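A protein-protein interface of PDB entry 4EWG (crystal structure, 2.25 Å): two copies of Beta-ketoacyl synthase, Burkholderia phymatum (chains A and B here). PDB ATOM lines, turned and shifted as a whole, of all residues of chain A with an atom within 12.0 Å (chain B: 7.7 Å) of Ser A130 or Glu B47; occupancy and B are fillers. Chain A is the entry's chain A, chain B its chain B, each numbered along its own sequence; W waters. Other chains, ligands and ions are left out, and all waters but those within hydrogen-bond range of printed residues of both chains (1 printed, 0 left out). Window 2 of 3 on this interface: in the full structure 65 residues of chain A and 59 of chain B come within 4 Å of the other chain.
No position is printed for both chains.
The backbone NH (N) of Ser A128 lies close to the side-chain hydroxyl (OH) of Tyr B45. O of Gly A129 is in hydrogen-bond range of N of Glu B47 (2.8 Å). The side-chain hydroxyl (OH) of Tyr B45 is in hydrogen-bond range of the backbone carbonyl oxygen (O) of Leu A126 (2.9 Å). The backbone NH of Ser B48 sits at hydrogen-bond distance from the side-chain sulfur of Met A131. N of Gly A129 sits at hydrogen-bond distance from OH of Tyr B45. The backbone carbonyl oxygen of Glu A127 sits at hydrogen-bond distance from the side-chain hydroxyl of Tyr B45 (3.1 Å). OE1 of Glu B47 sits at hydrogen-bond distance from N of Met A131, at 2.8 Å.
Among the printed residues, merely in contact across the chains: Met A125 with Phe B46 (3.5 Å), Thr A132 with Glu B47 (3.5 Å), Ser A130 with Glu B47 (3.6 Å), Gly A129 with Phe B46 (3.7 Å) and Met A125 with Tyr B45 (3.8 Å).
O of Thr A124 is in hydrogen-bond range of OG of Ser A128, at 3.2 Å. The side-chain hydroxyl of Ser A130 lies within hydrogen-bond range of the side-chain hydroxyl of Thr A132, at 3.2 Å. The side-chain hydroxyl (OG) of Ser A128 lies close to the backbone NH (N) of Ser A130, at 3.2 Å.
Of the printed residues of chain B, Met A125 touches Tyr B45 (3.8 Å) and Phe B46 (3.5 Å). Printed residues of chain B within 4 Å of Glu A127: Tyr B45. Of the printed residues of chain B, Ser A128 touches Tyr B45 (3.3 Å). Ser A130 touches just one residue of chain B: Glu B47. Of the printed residues of chain B, Met A131 touches Glu B47 and Ser B48. Tyr B45 touches just these residues of chain A: Met A125 (3.8 Å), Leu A126 (2.9 Å), Glu A127 (3.1 Å), Ser A128 (3.3 Å) and Gly A129 (3.3 Å). Of chain A, only Met A125 and Gly A129 come within 4 Å of Phe B46. Glu B47 touches just these residues of chain A: Gly A129, Ser A130, Met A131 and Thr A132. The nearest residue of chain B that does not touch Ser A130 is Tyr B45 (5.4 Å).
Water W1 lies within hydrogen-bond range of O of Tyr B45 (2.8 Å) and O of Ser A128 (3.0 Å).
Hydrophobic or aromatic side chains of chain A that line the printed part of chain B: Met A125 and Met A131.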
ATOM      1  N   GLU A 117     -11.856 -21.972   6.831  1.00  0.00           N
ATOM      2  CA  GLU A 117     -12.142 -20.886   7.766  1.00  0.00           C
ATOM      3  C   GLU A 117     -10.926 -19.982   7.996  1.00  0.00           C
ATOM      4  O   GLU A 117     -11.019 -18.783   7.813  1.00  0.00           O
ATOM      5  CB  GLU A 117     -12.680 -21.421   9.102  1.00  0.00           C
ATOM      6  CG  GLU A 117     -14.063 -22.043   8.996  1.00  0.00           C
ATOM      7  CD  GLU A 117     -14.094 -23.461   8.402  1.00  0.00           C
ATOM      8  OE1 GLU A 117     -13.004 -24.115   8.230  1.00  0.00           O
ATOM      9  OE2 GLU A 117     -15.238 -23.934   8.129  1.00  0.00           O
ATOM     10  N   PRO A 118      -9.781 -20.562   8.416  1.00  0.00           N
ATOM     11  CA  PRO A 118      -8.629 -19.712   8.707  1.00  0.00           C
ATOM     12  C   PRO A 118      -7.970 -19.125   7.460  1.00  0.00           C
ATOM     13  O   PRO A 118      -7.435 -18.005   7.530  1.00  0.00           O
ATOM     14  CB  PRO A 118      -7.673 -20.652   9.438  1.00  0.00           C
ATOM     15  CG  PRO A 118      -8.045 -22.007   8.924  1.00  0.00           C
ATOM     16  CD  PRO A 118      -9.533 -21.965   8.797  1.00  0.00           C
ATOM     17  N   ILE A 119      -8.032 -19.834   6.323  1.00  0.00           N
ATOM     18  CA  ILE A 119      -7.615 -19.235   5.068  1.00  0.00           C
ATOM     19  C   ILE A 119      -8.422 -17.957   4.815  1.00  0.00           C
ATOM     20  O   ILE A 119      -7.850 -16.923   4.505  1.00  0.00           O
ATOM     21  CB  ILE A 119      -7.724 -20.197   3.868  1.00  0.00           C
ATOM     22  CG1 ILE A 119      -6.731 -21.335   3.993  1.00  0.00           C
ATOM     23  CG2 ILE A 119      -7.385 -19.470   2.559  1.00  0.00           C
ATOM     24  CD1 ILE A 119      -7.059 -22.522   3.100  1.00  0.00           C
ATOM     25  N   ARG A 120      -9.735 -18.023   4.972  1.00  0.00           N
ATOM     26  CA  ARG A 120     -10.597 -16.835   4.884  1.00  0.00           C
ATOM     27  C   ARG A 120     -10.176 -15.750   5.880  1.00  0.00           C
ATOM     28  O   ARG A 120     -10.106 -14.567   5.535  1.00  0.00           O
ATOM     29  CB  ARG A 120     -12.081 -17.205   5.111  1.00  0.00           C
ATOM     30  CG  ARG A 120     -13.070 -16.049   4.840  1.00  0.00           C
ATOM     31  CD  ARG A 120     -14.533 -16.296   5.251  1.00  0.00           C
ATOM     32  NE  ARG A 120     -14.528 -17.122   6.430  1.00  0.00           N
ATOM     33  CZ  ARG A 120     -14.296 -16.684   7.669  1.00  0.00           C
ATOM     34  NH1 ARG A 120     -14.130 -15.377   7.921  1.00  0.00           N
ATOM     35  NH2 ARG A 120     -14.230 -17.581   8.674  1.00  0.00           N
ATOM     36  N   ALA A 121      -9.920 -16.163   7.120  1.00  0.00           N
ATOM     37  CA  ALA A 121      -9.629 -15.215   8.200  1.00  0.00           C
ATOM     38  C   ALA A 121      -8.297 -14.519   7.955  1.00  0.00           C
ATOM     39  O   ALA A 121      -8.204 -13.306   8.000  1.00  0.00           O
ATOM     40  CB  ALA A 121      -9.623 -15.924   9.552  1.00  0.00           C
ATOM     41  N   PHE A 122      -7.257 -15.289   7.698  1.00  0.00           N
ATOM     42  CA  PHE A 122      -5.931 -14.688   7.455  1.00  0.00           C
ATOM     43  C   PHE A 122      -5.873 -13.898   6.127  1.00  0.00           C
ATOM     44  O   PHE A 122      -5.250 -12.819   6.059  1.00  0.00           O
ATOM     45  CB  PHE A 122      -4.836 -15.753   7.485  1.00  0.00           C
ATOM     46  CG  PHE A 122      -4.453 -16.210   8.877  1.00  0.00           C
ATOM     47  CD1 PHE A 122      -4.007 -15.305   9.830  1.00  0.00           C
ATOM     48  CD2 PHE A 122      -4.486 -17.549   9.213  1.00  0.00           C
ATOM     49  CE1 PHE A 122      -3.609 -15.748  11.106  1.00  0.00           C
ATOM     50  CE2 PHE A 122      -4.117 -17.996  10.480  1.00  0.00           C
ATOM     51  CZ  PHE A 122      -3.666 -17.094  11.427  1.00  0.00           C
ATOM     52  N   GLY A 123      -6.519 -14.427   5.092  1.00  0.00           N
ATOM     53  CA  GLY A 123      -6.568 -13.759   3.794  1.00  0.00           C
ATOM     54  C   GLY A 123      -7.234 -12.411   3.900  1.00  0.00           C
ATOM     55  O   GLY A 123      -6.776 -11.442   3.318  1.00  0.00           O
ATOM     56  N   THR A 124      -8.309 -12.343   4.672  1.00  0.00           N
ATOM     57  CA  THR A 124      -8.994 -11.103   4.888  1.00  0.00           C
ATOM     58  C   THR A 124      -8.153 -10.128   5.751  1.00  0.00           C
ATOM     59  O   THR A 124      -8.216  -8.905   5.567  1.00  0.00           O
ATOM     60  CB  THR A 124     -10.379 -11.368   5.489  1.00  0.00           C
ATOM     61  OG1 THR A 124     -11.147 -12.108   4.534  1.00  0.00           O
ATOM     62  CG2 THR A 124     -11.101 -10.077   5.795  1.00  0.00           C
ATOM     63  N   MET A 125      -7.398 -10.658   6.703  1.00  0.00           N
ATOM     64  CA  MET A 125      -6.493  -9.835   7.477  1.00  0.00           C
ATOM     65  C   MET A 125      -5.544  -9.112   6.510  1.00  0.00           C
ATOM     66  O   MET A 125      -5.307  -7.930   6.656  1.00  0.00           O
ATOM     67  CB  MET A 125      -5.751 -10.695   8.531  1.00  0.00           C
ATOM     68  CG  MET A 125      -4.665  -9.969   9.331  1.00  0.00           C
ATOM     69  SD  MET A 125      -3.784 -11.039  10.469  1.00  0.00           S
ATOM     70  CE  MET A 125      -2.456  -9.973  10.968  1.00  0.00           C
ATOM     71  N   LEU A 126      -5.017  -9.831   5.521  1.00  0.00           N
ATOM     72  CA  LEU A 126      -4.198  -9.208   4.507  1.00  0.00           C
ATOM     73  C   LEU A 126      -5.019  -8.227   3.671  1.00  0.00           C
ATOM     74  O   LEU A 126      -4.589  -7.115   3.433  1.00  0.00           O
ATOM     75  CB  LEU A 126      -3.528 -10.259   3.617  1.00  0.00           C
ATOM     76  CG  LEU A 126      -2.466 -11.086   4.363  1.00  0.00           C
ATOM     77  CD1 LEU A 126      -2.161 -12.408   3.674  1.00  0.00           C
ATOM     78  CD2 LEU A 126      -1.223 -10.266   4.576  1.00  0.00           C
ATOM     79  N   GLU A 127      -6.206  -8.643   3.239  1.00  0.00           N
ATOM     80  CA  GLU A 127      -7.041  -7.835   2.351  1.00  0.00           C
ATOM     81  C   GLU A 127      -7.416  -6.473   2.939  1.00  0.00           C
ATOM     82  O   GLU A 127      -7.363  -5.476   2.230  1.00  0.00           O
ATOM     83  CB  GLU A 127      -8.339  -8.564   2.003  1.00  0.00           C
ATOM     84  CG  GLU A 127      -9.246  -7.802   1.032  1.00  0.00           C
ATOM     85  CD  GLU A 127      -8.545  -7.483  -0.276  1.00  0.00           C
ATOM     86  OE1 GLU A 127      -7.736  -8.310  -0.713  1.00  0.00           O
ATOM     87  OE2 GLU A 127      -8.795  -6.409  -0.883  1.00  0.00           O
ATOM     88  N   SER A 128      -7.808  -6.452   4.214  1.00  0.00           N
ATOM     89  CA  SER A 128      -8.354  -5.234   4.849  1.00  0.00           C
ATOM     90  C   SER A 128      -7.746  -4.877   6.230  1.00  0.00           C
ATOM     91  O   SER A 128      -8.111  -3.850   6.812  1.00  0.00           O
ATOM     92  CB  SER A 128      -9.851  -5.401   5.043  1.00  0.00           C
ATOM     93  OG  SER A 128     -10.103  -6.340   6.076  1.00  0.00           O
ATOM     94  N   GLY A 129      -6.854  -5.724   6.761  1.00  0.00           N
ATOM     95  CA  GLY A 129      -6.370  -5.540   8.138  1.00  0.00           C
ATOM     96  C   GLY A 129      -7.281  -6.077   9.250  1.00  0.00           C
ATOM     97  O   GLY A 129      -6.830  -6.255  10.397  1.00  0.00           O
ATOM     98  N   SER A 130      -8.542  -6.347   8.915  1.00  0.00           N
ATOM     99  CA  SER A 130      -9.494  -6.912   9.874  1.00  0.00           C
ATOM    100  C   SER A 130      -9.003  -8.259  10.464  1.00  0.00           C
ATOM    101  O   SER A 130      -8.549  -9.119   9.751  1.00  0.00           O
ATOM    102  CB  SER A 130     -10.854  -7.121   9.208  1.00  0.00           C
ATOM    103  OG  SER A 130     -11.657  -8.063   9.930  1.00  0.00           O
ATOM    104  N   MET A 131      -9.121  -8.405  11.780  1.00  0.00           N
ATOM    105  CA  MET A 131      -8.701  -9.622  12.470  1.00  0.00           C
ATOM    106  C   MET A 131      -9.841 -10.268  13.281  1.00  0.00           C
ATOM    107  O   MET A 131      -9.607 -11.103  14.187  1.00  0.00           O
ATOM    108  CB  MET A 131      -7.513  -9.307  13.351  1.00  0.00           C
ATOM    109  CG  MET A 131      -6.243  -9.163  12.545  1.00  0.00           C
ATOM    110  SD  MET A 131      -4.851  -8.646  13.576  1.00  0.00           S
ATOM    111  CE  MET A 131      -4.656 -10.062  14.679  1.00  0.00           C
ATOM    112  N   THR A 132     -11.073  -9.912  12.909  1.00  0.00           N
ATOM    113  CA  THR A 132     -12.270 -10.325  13.643  1.00  0.00           C
ATOM    114  C   THR A 132     -12.263 -11.807  13.887  1.00  0.00           C
ATOM    115  O   THR A 132     -12.476 -12.241  15.004  1.00  0.00           O
ATOM    116  CB  THR A 132     -13.569  -9.946  12.892  1.00  0.00           C
ATOM    117  OG1 THR A 132     -13.510  -8.565  12.501  1.00  0.00           O
ATOM    118  CG2 THR A 132     -14.819 -10.215  13.788  1.00  0.00           C
ATOM    119  N   ASP A 133     -12.011 -12.592  12.850  1.00  0.00           N
ATOM    120  CA  ASP A 133     -12.088 -14.035  12.974  1.00  0.00           C
ATOM    121  C   ASP A 133     -10.750 -14.713  13.041  1.00  0.00           C
ATOM    122  O   ASP A 133     -10.648 -15.930  12.873  1.00  0.00           O
ATOM    123  CB  ASP A 133     -12.862 -14.601  11.790  1.00  0.00           C
ATOM    124  CG  ASP A 133     -14.280 -14.076  11.722  1.00  0.00           C
ATOM    125  OD1 ASP A 133     -14.804 -13.626  12.739  1.00  0.00           O
ATOM    126  OD2 ASP A 133     -14.878 -14.144  10.641  1.00  0.00           O
ATOM    127  N   VAL A 134      -9.691 -13.953  13.253  1.00  0.00           N
ATOM    128  CA  VAL A 134      -8.390 -14.589  13.446  1.00  0.00           C
ATOM    129  C   VAL A 134      -8.335 -14.929  14.908  1.00  0.00           C
ATOM    130  O   VAL A 134      -8.447 -14.037  15.730  1.00  0.00           O
ATOM    131  CB  VAL A 134      -7.241 -13.634  13.043  1.00  0.00           C
ATOM    132  CG1 VAL A 134      -5.895 -14.158  13.532  1.00  0.00           C
ATOM    133  CG2 VAL A 134      -7.288 -13.392  11.539  1.00  0.00           C
ATOM    134  N   THR A 135      -8.187 -16.212  15.241  1.00  0.00           N
ATOM    135  CA  THR A 135      -8.023 -16.640  16.654  1.00  0.00           C
ATOM    136  C   THR A 135      -6.726 -17.379  16.879  1.00  0.00           C
ATOM    137  O   THR A 135      -5.959 -17.643  15.950  1.00  0.00           O
ATOM    138  CB  THR A 135      -9.166 -17.558  17.127  1.00  0.00           C
ATOM    139  OG1 THR A 135      -8.934 -18.904  16.676  1.00  0.00           O
ATOM    140  CG2 THR A 135     -10.529 -17.025  16.647  1.00  0.00           C
ATOM    141  N   SER A 138      -6.470 -20.497  14.656  1.00  0.00           N
ATOM    142  CA  SER A 138      -6.544 -20.390  13.193  1.00  0.00           C
ATOM    143  C   SER A 138      -5.345 -21.063  12.505  1.00  0.00           C
ATOM    144  O   SER A 138      -5.502 -21.840  11.538  1.00  0.00           O
ATOM    145  CB  SER A 138      -6.667 -18.915  12.789  1.00  0.00           C
ATOM    146  OG  SER A 138      -7.906 -18.349  13.224  1.00  0.00           O
ATOM    147  N   TRP B  43       2.494  -2.131  10.693  1.00  0.00           N
ATOM    148  CA  TRP B  43       1.557  -3.068  11.324  1.00  0.00           C
ATOM    149  C   TRP B  43       0.419  -2.425  12.041  1.00  0.00           C
ATOM    150  O   TRP B  43      -0.475  -3.142  12.517  1.00  0.00           O
ATOM    151  CB  TRP B  43       2.301  -4.000  12.259  1.00  0.00           C
ATOM    152  CG  TRP B  43       3.138  -4.989  11.512  1.00  0.00           C
ATOM    153  CD1 TRP B  43       3.163  -5.227  10.115  1.00  0.00           C
ATOM    154  CD2 TRP B  43       4.047  -5.951  12.083  1.00  0.00           C
ATOM    155  NE1 TRP B  43       4.045  -6.234   9.817  1.00  0.00           N
ATOM    156  CE2 TRP B  43       4.597  -6.723  10.963  1.00  0.00           C
ATOM    157  CE3 TRP B  43       4.459  -6.239  13.357  1.00  0.00           C
ATOM    158  CZ2 TRP B  43       5.522  -7.738  11.160  1.00  0.00           C
ATOM    159  CZ3 TRP B  43       5.391  -7.249  13.546  1.00  0.00           C
ATOM    160  CH2 TRP B  43       5.906  -7.991  12.480  1.00  0.00           C
ATOM    161  N   ASP B  44       0.405  -1.084  12.122  1.00  0.00           N
ATOM    162  CA  ASP B  44      -0.795  -0.364  12.563  1.00  0.00           C
ATOM    163  C   ASP B  44      -1.972  -0.586  11.588  1.00  0.00           C
ATOM    164  O   ASP B  44      -3.127  -0.331  11.909  1.00  0.00           O
ATOM    165  CB  ASP B  44      -0.535   1.125  12.660  1.00  0.00           C
ATOM    166  CG  ASP B  44       0.518   1.479  13.704  1.00  0.00           C
ATOM    167  OD1 ASP B  44       0.972   0.610  14.469  1.00  0.00           O
ATOM    168  OD2 ASP B  44       0.919   2.656  13.724  1.00  0.00           O
ATOM    169  N   TYR B  45      -1.655  -1.034  10.384  1.00  0.00           N
ATOM    170  CA  TYR B  45      -2.659  -1.466   9.447  1.00  0.00           C
ATOM    171  C   TYR B  45      -3.531  -2.593  10.047  1.00  0.00           C
ATOM    172  O   TYR B  45      -4.710  -2.675   9.768  1.00  0.00           O
ATOM    173  CB  TYR B  45      -1.953  -1.950   8.171  1.00  0.00           C
ATOM    174  CG  TYR B  45      -2.848  -2.598   7.115  1.00  0.00           C
ATOM    175  CD1 TYR B  45      -3.575  -1.820   6.217  1.00  0.00           C
ATOM    176  CD2 TYR B  45      -2.928  -3.992   7.004  1.00  0.00           C
ATOM    177  CE1 TYR B  45      -4.381  -2.408   5.244  1.00  0.00           C
ATOM    178  CE2 TYR B  45      -3.717  -4.589   6.032  1.00  0.00           C
ATOM    179  CZ  TYR B  45      -4.447  -3.794   5.164  1.00  0.00           C
ATOM    180  OH  TYR B  45      -5.236  -4.392   4.216  1.00  0.00           O
ATOM    181  N   PHE B  46      -2.929  -3.470  10.848  1.00  0.00           N
ATOM    182  CA  PHE B  46      -3.637  -4.660  11.321  1.00  0.00           C
ATOM    183  C   PHE B  46      -4.459  -4.329  12.527  1.00  0.00           C
ATOM    184  O   PHE B  46      -4.067  -3.514  13.354  1.00  0.00           O
ATOM    185  CB  PHE B  46      -2.676  -5.807  11.582  1.00  0.00           C
ATOM    186  CG  PHE B  46      -2.006  -6.298  10.339  1.00  0.00           C
ATOM    187  CD1 PHE B  46      -2.761  -6.903   9.322  1.00  0.00           C
ATOM    188  CD2 PHE B  46      -0.642  -6.140  10.151  1.00  0.00           C
ATOM    189  CE1 PHE B  46      -2.162  -7.327   8.160  1.00  0.00           C
ATOM    190  CE2 PHE B  46      -0.040  -6.580   8.976  1.00  0.00           C
ATOM    191  CZ  PHE B  46      -0.799  -7.176   7.986  1.00  0.00           C
ATOM    192  N   GLU B  47      -5.638  -4.939  12.606  1.00  0.00           N
ATOM    193  CA  GLU B  47      -6.629  -4.526  13.595  1.00  0.00           C
ATOM    194  C   GLU B  47      -6.081  -4.703  15.025  1.00  0.00           C
ATOM    195  O   GLU B  47      -6.045  -3.760  15.781  1.00  0.00           O
ATOM    196  CB  GLU B  47      -7.954  -5.293  13.399  1.00  0.00           C
ATOM    197  CG  GLU B  47      -9.147  -4.595  14.028  1.00  0.00           C
ATOM    198  CD  GLU B  47     -10.467  -5.351  13.854  1.00  0.00           C
ATOM    199  OE1 GLU B  47     -10.475  -6.459  13.297  1.00  0.00           O
ATOM    200  OE2 GLU B  47     -11.505  -4.830  14.304  1.00  0.00           O
ATOM    201  N   SER B  48      -5.616  -5.909  15.357  1.00  0.00           N
ATOM    202  CA  SER B  48      -5.376  -6.308  16.756  1.00  0.00           C
ATOM    203  C   SER B  48      -4.043  -7.052  17.005  1.00  0.00           C
ATOM    204  O   SER B  48      -4.050  -8.161  17.511  1.00  0.00           O
ATOM    205  CB  SER B  48      -6.512  -7.233  17.180  1.00  0.00           C
ATOM    206  OG  SER B  48      -7.749  -6.773  16.698  1.00  0.00           O
ATOM    207  N   LEU B  49      -2.925  -6.474  16.597  1.00  0.00           N
ATOM    208  CA  LEU B  49      -1.604  -7.008  16.943  1.00  0.00           C
ATOM    209  C   LEU B  49      -1.074  -6.181  18.068  1.00  0.00           C
ATOM    210  O   LEU B  49      -1.126  -4.975  17.994  1.00  0.00           O
ATOM    211  CB  LEU B  49      -0.631  -6.919  15.769  1.00  0.00           C
ATOM    212  CG  LEU B  49      -0.702  -7.963  14.671  1.00  0.00           C
ATOM    213  CD1 LEU B  49       0.289  -7.559  13.576  1.00  0.00           C
ATOM    214  CD2 LEU B  49      -0.386  -9.361  15.185  1.00  0.00           C
ATOM    215  N   HIS B  50      -0.587  -6.830  19.110  1.00  0.00           N
ATOM    216  CA  HIS B  50      -0.008  -6.133  20.249  1.00  0.00           C
ATOM    217  C   HIS B  50       1.398  -5.762  19.931  1.00  0.00           C
ATOM    218  O   HIS B  50       1.809  -4.638  20.194  1.00  0.00           O
ATOM    219  CB  HIS B  50      -0.037  -7.010  21.508  1.00  0.00           C
ATOM    220  CG  HIS B  50      -1.432  -7.274  22.037  1.00  0.00           C
ATOM    221  ND1 HIS B  50      -2.183  -8.299  21.609  1.00  0.00           N
ATOM    222  CD2 HIS B  50      -2.201  -6.593  22.972  1.00  0.00           C
ATOM    223  CE1 HIS B  50      -3.357  -8.284  22.225  1.00  0.00           C
ATOM    224  NE2 HIS B  50      -3.377  -7.229  23.051  1.00  0.00           N
ATOM    225  N   ARG B  52       4.715  -4.654  17.952  1.00  0.00           N
ATOM    226  CA  ARG B  52       5.177  -3.870  16.817  1.00  0.00           C
ATOM    227  C   ARG B  52       6.662  -4.155  16.555  1.00  0.00           C
ATOM    228  O   ARG B  52       7.394  -3.294  16.069  1.00  0.00           O
ATOM    229  CB  ARG B  52       4.959  -2.374  17.072  1.00  0.00           C
ATOM    230  CG  ARG B  52       3.506  -1.959  17.115  1.00  0.00           C
ATOM    231  CD  ARG B  52       2.897  -2.055  15.721  1.00  0.00           C
ATOM    232  NE  ARG B  52       1.496  -1.672  15.691  1.00  0.00           N
ATOM    233  CZ  ARG B  52       0.489  -2.488  15.937  1.00  0.00           C
ATOM    234  NH1 ARG B  52       0.698  -3.775  16.222  1.00  0.00           N
ATOM    235  NH2 ARG B  52      -0.740  -2.024  15.894  1.00  0.00           N
HETATM  236  O   HOH W   1      -6.542  -1.576   7.964  1.00  0.00           O
